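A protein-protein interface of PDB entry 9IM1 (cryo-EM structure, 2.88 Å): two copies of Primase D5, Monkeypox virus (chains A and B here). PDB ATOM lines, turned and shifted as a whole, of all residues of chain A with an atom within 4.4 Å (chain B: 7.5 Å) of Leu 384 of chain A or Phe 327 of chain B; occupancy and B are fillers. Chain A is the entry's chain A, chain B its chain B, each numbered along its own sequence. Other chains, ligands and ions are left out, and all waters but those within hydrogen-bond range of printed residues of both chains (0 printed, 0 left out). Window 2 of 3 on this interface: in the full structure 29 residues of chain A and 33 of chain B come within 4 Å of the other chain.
OD1 of Asn 395 of chain B is in hydrogen-bond range of NH2 of Arg 389 of chain A (3.0 Å). NE of Arg 389 of chain A is in salt-bridge range of OD2 of Asp 398 of chain B (3.0 Å).
O of Leu 369 of chain A lies within hydrogen-bond range of NH1 of Arg 372 of chain A (2.7 Å). O of Asn 324 of chain B lies within hydrogen-bond range of ND2 of Asn 328 of chain B (2.9 Å). O of Leu 383 of chain A lies within hydrogen-bond range of NH1 of Arg 389 of chain A (2.9 Å). N of Leu 326 of chain B lies within hydrogen-bond range of OD1 of Asn 324 of chain B (2.6 Å). The side-chain amide oxygen (OD1) of Asn 324 of chain B sits at hydrogen-bond distance from the backbone NH (N) of Phe 327 of chain B (2.6 Å).
Phe 327 of chain B touches Leu 369 of chain A (CE1 to CD1, 3.9 Å). O of Leu 384 of chain A touches ND2 of Asn 324 of chain B, at 3.9 Å. Phe 327 of chain B touches Leu 384 of chain A (CE1 to CD2, 3.7 Å). CG of Pro 386 of chain A touches OD1 of Asn 395 of chain B (3.9 Å).
Of the printed residues of chain B, Leu 369 of chain A touches Phe 327. Of chain B, only Asn 324 (3.9 Å) and Phe 327 (3.7 Å) come within 4 Å of Leu 384 of chain A. Of the printed residues of chain B, Pro 386 of chain A touches Asn 395 (3.9 Å). Printed residues of chain B within 4 Å of Arg 389 of chain A: Asn 395 (3.0 Å) and Asp 398 (2.4 Å). Of the printed residues of chain A, Asn 395 of chain B touches Pro 386 (3.9 Å) and Arg 389 (3.0 Å). Of the printed residues of chain A, Asp 398 of chain B touches Arg 389 (2.4 Å). The nearest residue of chain B that does not touch Leu 384 of chain A is Asn 395 of chain B (4.2 Å). The nearest residue of chain A that does not touch Phe 327 of chain B is Arg 372 of chain A (4.1 Å).
Of the 17 printed residues of chain B, 4 touch a printed residue of chain A. Printed residues of chain B that touch a printed residue of chain A: Asn 324, Phe 327, Asn 395 and Asp 398. Along chain B the printed residues that touch a printed residue of chain A span positions 324 to 398. Of the 9 printed residues of chain A, 4 touch a printed residue of chain B. Among the printed residues, Asp or Glu carboxylates within 4 Å of a Lys or Arg side-chain nitrogen of the other chain: Arg 389 of chain A with Asp 398 of chain B (2.4 Å).
No position is printed for both chains. Of the 6 pairs that touch across the chains among the printed residues, none has its exchanged pair printed and touching as well.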
ATOM      1  N   LEU A 369      13.476  12.259  -1.651  1.00  0.00           N
ATOM      2  CA  LEU A 369      13.303  10.978  -0.976  1.00  0.00           C
ATOM      3  C   LEU A 369      14.423  10.723   0.024  1.00  0.00           C
ATOM      4  O   LEU A 369      14.183  10.178   1.107  1.00  0.00           O
ATOM      5  CB  LEU A 369      13.230   9.848  -2.002  1.00  0.00           C
ATOM      6  CG  LEU A 369      12.959   8.443  -1.457  1.00  0.00           C
ATOM      7  CD1 LEU A 369      11.931   7.732  -2.313  1.00  0.00           C
ATOM      8  CD2 LEU A 369      14.239   7.630  -1.391  1.00  0.00           C
ATOM      9  N   ARG A 372      14.588  12.754   3.641  1.00  0.00           N
ATOM     10  CA  ARG A 372      13.388  12.683   4.470  1.00  0.00           C
ATOM     11  C   ARG A 372      13.683  12.366   5.931  1.00  0.00           C
ATOM     12  O   ARG A 372      12.790  12.531   6.768  1.00  0.00           O
ATOM     13  CB  ARG A 372      12.414  11.641   3.918  1.00  0.00           C
ATOM     14  CG  ARG A 372      12.795  10.203   4.214  1.00  0.00           C
ATOM     15  CD  ARG A 372      11.874   9.235   3.492  1.00  0.00           C
ATOM     16  NE  ARG A 372      12.197   7.844   3.782  1.00  0.00           N
ATOM     17  CZ  ARG A 372      13.163   7.159   3.185  1.00  0.00           C
ATOM     18  NH1 ARG A 372      13.926   7.707   2.255  1.00  0.00           N
ATOM     19  NH2 ARG A 372      13.365   5.891   3.529  1.00  0.00           N
ATOM     20  N   SER A 381       6.482  11.084   6.897  1.00  0.00           N
ATOM     21  CA  SER A 381       5.489  10.154   6.372  1.00  0.00           C
ATOM     22  C   SER A 381       4.808  10.658   5.106  1.00  0.00           C
ATOM     23  O   SER A 381       4.164   9.863   4.412  1.00  0.00           O
ATOM     24  CB  SER A 381       4.430   9.860   7.433  1.00  0.00           C
ATOM     25  OG  SER A 381       3.439   8.984   6.926  1.00  0.00           O
ATOM     26  N   GLU A 382       4.924  11.948   4.794  1.00  0.00           N
ATOM     27  CA  GLU A 382       4.253  12.535   3.641  1.00  0.00           C
ATOM     28  C   GLU A 382       5.010  12.344   2.335  1.00  0.00           C
ATOM     29  O   GLU A 382       4.433  12.574   1.268  1.00  0.00           O
ATOM     30  CB  GLU A 382       4.031  14.030   3.881  1.00  0.00           C
ATOM     31  CG  GLU A 382       2.729  14.368   4.582  1.00  0.00           C
ATOM     32  CD  GLU A 382       1.568  13.533   4.087  1.00  0.00           C
ATOM     33  OE1 GLU A 382       1.280  13.581   2.874  1.00  0.00           O
ATOM     34  OE2 GLU A 382       0.943  12.830   4.909  1.00  0.00           O
ATOM     35  N   LEU A 383       6.273  11.930   2.384  1.00  0.00           N
ATOM     36  CA  LEU A 383       7.129  11.906   1.206  1.00  0.00           C
ATOM     37  C   LEU A 383       7.234  10.526   0.573  1.00  0.00           C
ATOM     38  O   LEU A 383       8.096  10.318  -0.287  1.00  0.00           O
ATOM     39  CB  LEU A 383       8.522  12.424   1.562  1.00  0.00           C
ATOM     40  CG  LEU A 383       8.599  13.900   1.954  1.00  0.00           C
ATOM     41  CD1 LEU A 383      10.042  14.333   2.121  1.00  0.00           C
ATOM     42  CD2 LEU A 383       7.896  14.760   0.918  1.00  0.00           C
ATOM     43  N   LEU A 384       6.389   9.583   0.973  1.00  0.00           N
ATOM     44  CA  LEU A 384       6.423   8.238   0.418  1.00  0.00           C
ATOM     45  C   LEU A 384       5.550   8.080  -0.820  1.00  0.00           C
ATOM     46  O   LEU A 384       5.552   7.004  -1.426  1.00  0.00           O
ATOM     47  CB  LEU A 384       6.003   7.221   1.481  1.00  0.00           C
ATOM     48  CG  LEU A 384       6.877   7.178   2.736  1.00  0.00           C
ATOM     49  CD1 LEU A 384       6.539   5.968   3.587  1.00  0.00           C
ATOM     50  CD2 LEU A 384       8.350   7.183   2.367  1.00  0.00           C
ATOM     51  N   CYS A 385       4.810   9.117  -1.215  1.00  0.00           N
ATOM     52  CA  CYS A 385       3.979   9.036  -2.410  1.00  0.00           C
ATOM     53  C   CYS A 385       4.635   9.797  -3.548  1.00  0.00           C
ATOM     54  O   CYS A 385       5.041  10.952  -3.356  1.00  0.00           O
ATOM     55  CB  CYS A 385       2.590   9.605  -2.141  1.00  0.00           C
ATOM     56  SG  CYS A 385       1.395   9.310  -3.463  1.00  0.00           S
ATOM     57  N   PRO A 386       4.772   9.189  -4.730  1.00  0.00           N
ATOM     58  CA  PRO A 386       5.452   9.889  -5.834  1.00  0.00           C
ATOM     59  C   PRO A 386       4.789  11.195  -6.239  1.00  0.00           C
ATOM     60  O   PRO A 386       5.490  12.153  -6.585  1.00  0.00           O
ATOM     61  CB  PRO A 386       5.419   8.857  -6.970  1.00  0.00           C
ATOM     62  CG  PRO A 386       5.214   7.542  -6.296  1.00  0.00           C
ATOM     63  CD  PRO A 386       4.370   7.824  -5.099  1.00  0.00           C
ATOM     64  N   ARG A 389       5.858  13.995  -4.050  1.00  0.00           N
ATOM     65  CA  ARG A 389       7.224  14.375  -4.387  1.00  0.00           C
ATOM     66  C   ARG A 389       7.262  15.234  -5.645  1.00  0.00           C
ATOM     67  O   ARG A 389       8.043  16.187  -5.725  1.00  0.00           O
ATOM     68  CB  ARG A 389       8.092  13.129  -4.549  1.00  0.00           C
ATOM     69  CG  ARG A 389       8.224  12.312  -3.277  1.00  0.00           C
ATOM     70  CD  ARG A 389       9.496  11.488  -3.276  1.00  0.00           C
ATOM     71  NE  ARG A 389       9.435  10.396  -4.238  1.00  0.00           N
ATOM     72  CZ  ARG A 389       9.064   9.159  -3.943  1.00  0.00           C
ATOM     73  NH1 ARG A 389       8.709   8.819  -2.715  1.00  0.00           N
ATOM     74  NH2 ARG A 389       9.047   8.240  -4.902  1.00  0.00           N
ATOM     75  N   GLY B 323       2.566   3.385   7.360  1.00  0.00           N
ATOM     76  CA  GLY B 323       3.418   2.619   6.472  1.00  0.00           C
ATOM     77  C   GLY B 323       2.794   2.366   5.113  1.00  0.00           C
ATOM     78  O   GLY B 323       1.811   1.637   4.997  1.00  0.00           O
ATOM     79  N   ASN B 324       3.368   2.977   4.082  1.00  0.00           N
ATOM     80  CA  ASN B 324       2.863   2.796   2.729  1.00  0.00           C
ATOM     81  C   ASN B 324       3.190   1.387   2.253  1.00  0.00           C
ATOM     82  O   ASN B 324       4.332   0.930   2.367  1.00  0.00           O
ATOM     83  CB  ASN B 324       3.466   3.861   1.805  1.00  0.00           C
ATOM     84  CG  ASN B 324       3.160   3.631   0.329  1.00  0.00           C
ATOM     85  OD1 ASN B 324       3.381   2.551  -0.219  1.00  0.00           O
ATOM     86  ND2 ASN B 324       2.644   4.666  -0.321  1.00  0.00           N
ATOM     87  N   LYS B 325       2.183   0.695   1.717  1.00  0.00           N
ATOM     88  CA  LYS B 325       2.369  -0.689   1.295  1.00  0.00           C
ATOM     89  C   LYS B 325       3.247  -0.777   0.053  1.00  0.00           C
ATOM     90  O   LYS B 325       4.171  -1.599  -0.013  1.00  0.00           O
ATOM     91  CB  LYS B 325       1.007  -1.336   1.042  1.00  0.00           C
ATOM     92  CG  LYS B 325       1.068  -2.688   0.360  1.00  0.00           C
ATOM     93  CD  LYS B 325       0.301  -3.736   1.149  1.00  0.00           C
ATOM     94  CE  LYS B 325      -1.057  -3.216   1.588  1.00  0.00           C
ATOM     95  NZ  LYS B 325      -2.008  -3.125   0.448  1.00  0.00           N
ATOM     96  N   LEU B 326       2.974   0.067  -0.944  1.00  0.00           N
ATOM     97  CA  LEU B 326       3.739   0.023  -2.186  1.00  0.00           C
ATOM     98  C   LEU B 326       5.200   0.382  -1.955  1.00  0.00           C
ATOM     99  O   LEU B 326       6.084  -0.166  -2.621  1.00  0.00           O
ATOM    100  CB  LEU B 326       3.109   0.960  -3.215  1.00  0.00           C
ATOM    101  CG  LEU B 326       1.734   0.525  -3.727  1.00  0.00           C
ATOM    102  CD1 LEU B 326       1.210   1.496  -4.771  1.00  0.00           C
ATOM    103  CD2 LEU B 326       1.785  -0.887  -4.286  1.00  0.00           C
ATOM    104  N   PHE B 327       5.472   1.292  -1.017  1.00  0.00           N
ATOM    105  CA  PHE B 327       6.853   1.596  -0.664  1.00  0.00           C
ATOM    106  C   PHE B 327       7.555   0.370  -0.093  1.00  0.00           C
ATOM    107  O   PHE B 327       8.718   0.098  -0.421  1.00  0.00           O
ATOM    108  CB  PHE B 327       6.892   2.751   0.332  1.00  0.00           C
ATOM    109  CG  PHE B 327       8.226   3.424   0.428  1.00  0.00           C
ATOM    110  CD1 PHE B 327       8.557   4.458  -0.428  1.00  0.00           C
ATOM    111  CD2 PHE B 327       9.148   3.028   1.378  1.00  0.00           C
ATOM    112  CE1 PHE B 327       9.783   5.080  -0.340  1.00  0.00           C
ATOM    113  CE2 PHE B 327      10.376   3.647   1.470  1.00  0.00           C
ATOM    114  CZ  PHE B 327      10.693   4.675   0.611  1.00  0.00           C
ATOM    115  N   ASN B 328       6.863  -0.383   0.763  1.00  0.00           N
ATOM    116  CA  ASN B 328       7.447  -1.607   1.301  1.00  0.00           C
ATOM    117  C   ASN B 328       7.715  -2.618   0.195  1.00  0.00           C
ATOM    118  O   ASN B 328       8.764  -3.273   0.188  1.00  0.00           O
ATOM    119  CB  ASN B 328       6.528  -2.208   2.362  1.00  0.00           C
ATOM    120  CG  ASN B 328       6.309  -1.278   3.534  1.00  0.00           C
ATOM    121  OD1 ASN B 328       7.226  -0.587   3.973  1.00  0.00           O
ATOM    122  ND2 ASN B 328       5.087  -1.258   4.051  1.00  0.00           N
ATOM    123  N   ILE B 329       6.780  -2.760  -0.747  1.00  0.00           N
ATOM    124  CA  ILE B 329       6.992  -3.683  -1.860  1.00  0.00           C
ATOM    125  C   ILE B 329       8.211  -3.268  -2.670  1.00  0.00           C
ATOM    126  O   ILE B 329       9.034  -4.109  -3.059  1.00  0.00           O
ATOM    127  CB  ILE B 329       5.732  -3.767  -2.740  1.00  0.00           C
ATOM    128  CG1 ILE B 329       4.507  -4.103  -1.889  1.00  0.00           C
ATOM    129  CG2 ILE B 329       5.929  -4.785  -3.849  1.00  0.00           C
ATOM    130  CD1 ILE B 329       3.401  -4.803  -2.645  1.00  0.00           C
ATOM    131  N   ALA B 330       8.347  -1.969  -2.939  1.00  0.00           N
ATOM    132  CA  ALA B 330       9.503  -1.483  -3.682  1.00  0.00           C
ATOM    133  C   ALA B 330      10.798  -1.770  -2.935  1.00  0.00           C
ATOM    134  O   ALA B 330      11.799  -2.166  -3.543  1.00  0.00           O
ATOM    135  CB  ALA B 330       9.362   0.013  -3.955  1.00  0.00           C
ATOM    136  N   GLN B 331      10.800  -1.576  -1.615  1.00  0.00           N
ATOM    137  CA  GLN B 331      12.006  -1.846  -0.836  1.00  0.00           C
ATOM    138  C   GLN B 331      12.374  -3.325  -0.869  1.00  0.00           C
ATOM    139  O   GLN B 331      13.550  -3.675  -1.033  1.00  0.00           O
ATOM    140  CB  GLN B 331      11.818  -1.372   0.603  1.00  0.00           C
ATOM    141  CG  GLN B 331      13.091  -1.415   1.428  1.00  0.00           C
ATOM    142  CD  GLN B 331      14.018  -0.258   1.124  1.00  0.00           C
ATOM    143  OE1 GLN B 331      15.039  -0.424   0.456  1.00  0.00           O
ATOM    144  NE2 GLN B 331      13.668   0.924   1.613  1.00  0.00           N
ATOM    145  N   ARG B 332      11.385  -4.209  -0.717  1.00  0.00           N
ATOM    146  CA  ARG B 332      11.677  -5.640  -0.757  1.00  0.00           C
ATOM    147  C   ARG B 332      12.179  -6.064  -2.130  1.00  0.00           C
ATOM    148  O   ARG B 332      13.067  -6.919  -2.235  1.00  0.00           O
ATOM    149  CB  ARG B 332      10.449  -6.459  -0.359  1.00  0.00           C
ATOM    150  CG  ARG B 332       9.769  -5.988   0.909  1.00  0.00           C
ATOM    151  CD  ARG B 332      10.099  -6.877   2.090  1.00  0.00           C
ATOM    152  NE  ARG B 332       9.647  -8.248   1.891  1.00  0.00           N
ATOM    153  CZ  ARG B 332       8.772  -8.865   2.672  1.00  0.00           C
ATOM    154  NH1 ARG B 332       8.215  -8.254   3.704  1.00  0.00           N
ATOM    155  NH2 ARG B 332       8.446 -10.127   2.410  1.00  0.00           N
ATOM    156  N   ILE B 333      11.617  -5.490  -3.195  1.00  0.00           N
ATOM    157  CA  ILE B 333      12.104  -5.800  -4.537  1.00  0.00           C
ATOM    158  C   ILE B 333      13.538  -5.319  -4.708  1.00  0.00           C
ATOM    159  O   ILE B 333      14.387  -6.032  -5.257  1.00  0.00           O
ATOM    160  CB  ILE B 333      11.169  -5.194  -5.600  1.00  0.00           C
ATOM    161  CG1 ILE B 333       9.869  -5.992  -5.680  1.00  0.00           C
ATOM    162  CG2 ILE B 333      11.850  -5.168  -6.955  1.00  0.00           C
ATOM    163  CD1 ILE B 333       8.865  -5.419  -6.648  1.00  0.00           C
ATOM    164  N   TYR B 379       0.785  -9.139  -0.430  1.00  0.00           N
ATOM    165  CA  TYR B 379       1.438  -8.242  -1.373  1.00  0.00           C
ATOM    166  C   TYR B 379       1.232  -8.647  -2.823  1.00  0.00           C
ATOM    167  O   TYR B 379       1.285  -7.787  -3.708  1.00  0.00           O
ATOM    168  CB  TYR B 379       2.944  -8.181  -1.094  1.00  0.00           C
ATOM    169  CG  TYR B 379       3.331  -7.391   0.133  1.00  0.00           C
ATOM    170  CD1 TYR B 379       2.377  -6.745   0.903  1.00  0.00           C
ATOM    171  CD2 TYR B 379       4.660  -7.293   0.522  1.00  0.00           C
ATOM    172  CE1 TYR B 379       2.735  -6.023   2.024  1.00  0.00           C
ATOM    173  CE2 TYR B 379       5.026  -6.574   1.640  1.00  0.00           C
ATOM    174  CZ  TYR B 379       4.060  -5.940   2.387  1.00  0.00           C
ATOM    175  OH  TYR B 379       4.417  -5.221   3.503  1.00  0.00           O
ATOM    176  N   THR B 391       3.465   2.829 -10.098  1.00  0.00           N
ATOM    177  CA  THR B 391       3.866   3.491  -8.858  1.00  0.00           C
ATOM    178  C   THR B 391       5.106   2.836  -8.255  1.00  0.00           C
ATOM    179  O   THR B 391       6.043   3.525  -7.823  1.00  0.00           O
ATOM    180  CB  THR B 391       2.713   3.469  -7.856  1.00  0.00           C
ATOM    181  OG1 THR B 391       1.592   4.174  -8.403  1.00  0.00           O
ATOM    182  CG2 THR B 391       3.129   4.129  -6.555  1.00  0.00           C
ATOM    183  N   VAL B 392       5.135   1.503  -8.230  1.00  0.00           N
ATOM    184  CA  VAL B 392       6.305   0.799  -7.711  1.00  0.00           C
ATOM    185  C   VAL B 392       7.520   1.068  -8.590  1.00  0.00           C
ATOM    186  O   VAL B 392       8.647   1.192  -8.096  1.00  0.00           O
ATOM    187  CB  VAL B 392       6.013  -0.707  -7.584  1.00  0.00           C
ATOM    188  CG1 VAL B 392       7.236  -1.445  -7.077  1.00  0.00           C
ATOM    189  CG2 VAL B 392       4.841  -0.937  -6.652  1.00  0.00           C
ATOM    190  N   ASN B 395       8.884   4.422  -7.592  1.00  0.00           N
ATOM    191  CA  ASN B 395       9.652   4.306  -6.353  1.00  0.00           C
ATOM    192  C   ASN B 395      11.024   3.690  -6.608  1.00  0.00           C
ATOM    193  O   ASN B 395      12.042   4.201  -6.126  1.00  0.00           O
ATOM    194  CB  ASN B 395       8.877   3.483  -5.326  1.00  0.00           C
ATOM    195  CG  ASN B 395       7.824   4.295  -4.609  1.00  0.00           C
ATOM    196  OD1 ASN B 395       7.957   5.508  -4.463  1.00  0.00           O
ATOM    197  ND2 ASN B 395       6.770   3.631  -4.153  1.00  0.00           N
ATOM    198  N   ASP B 398      13.314   6.009  -8.061  1.00  0.00           N
ATOM    199  CA  ASP B 398      13.740   7.001  -7.081  1.00  0.00           C
ATOM    200  C   ASP B 398      14.813   6.468  -6.139  1.00  0.00           C
ATOM    201  O   ASP B 398      15.630   7.251  -5.641  1.00  0.00           O
ATOM    202  CB  ASP B 398      12.537   7.494  -6.278  1.00  0.00           C
ATOM    203  CG  ASP B 398      11.757   8.568  -7.002  1.00  0.00           C
ATOM    204  OD1 ASP B 398      12.277   9.108  -8.001  1.00  0.00           O
ATOM    205  OD2 ASP B 398      10.622   8.866  -6.581  1.00  0.00           O
ATOM    206  N   MET B 399      14.836   5.163  -5.870  1.00  0.00           N
ATOM    207  CA  MET B 399      15.793   4.623  -4.906  1.00  0.00           C
ATOM    208  C   MET B 399      17.122   4.202  -5.522  1.00  0.00           C
ATOM    209  O   MET B 399      18.033   3.827  -4.781  1.00  0.00           O
ATOM    210  CB  MET B 399      15.205   3.424  -4.156  1.00  0.00           C
ATOM    211  CG  MET B 399      13.763   3.560  -3.745  1.00  0.00           C
ATOM    212  SD  MET B 399      13.109   1.998  -3.136  1.00  0.00           S
ATOM    213  CE  MET B 399      12.128   2.566  -1.756  1.00  0.00           C
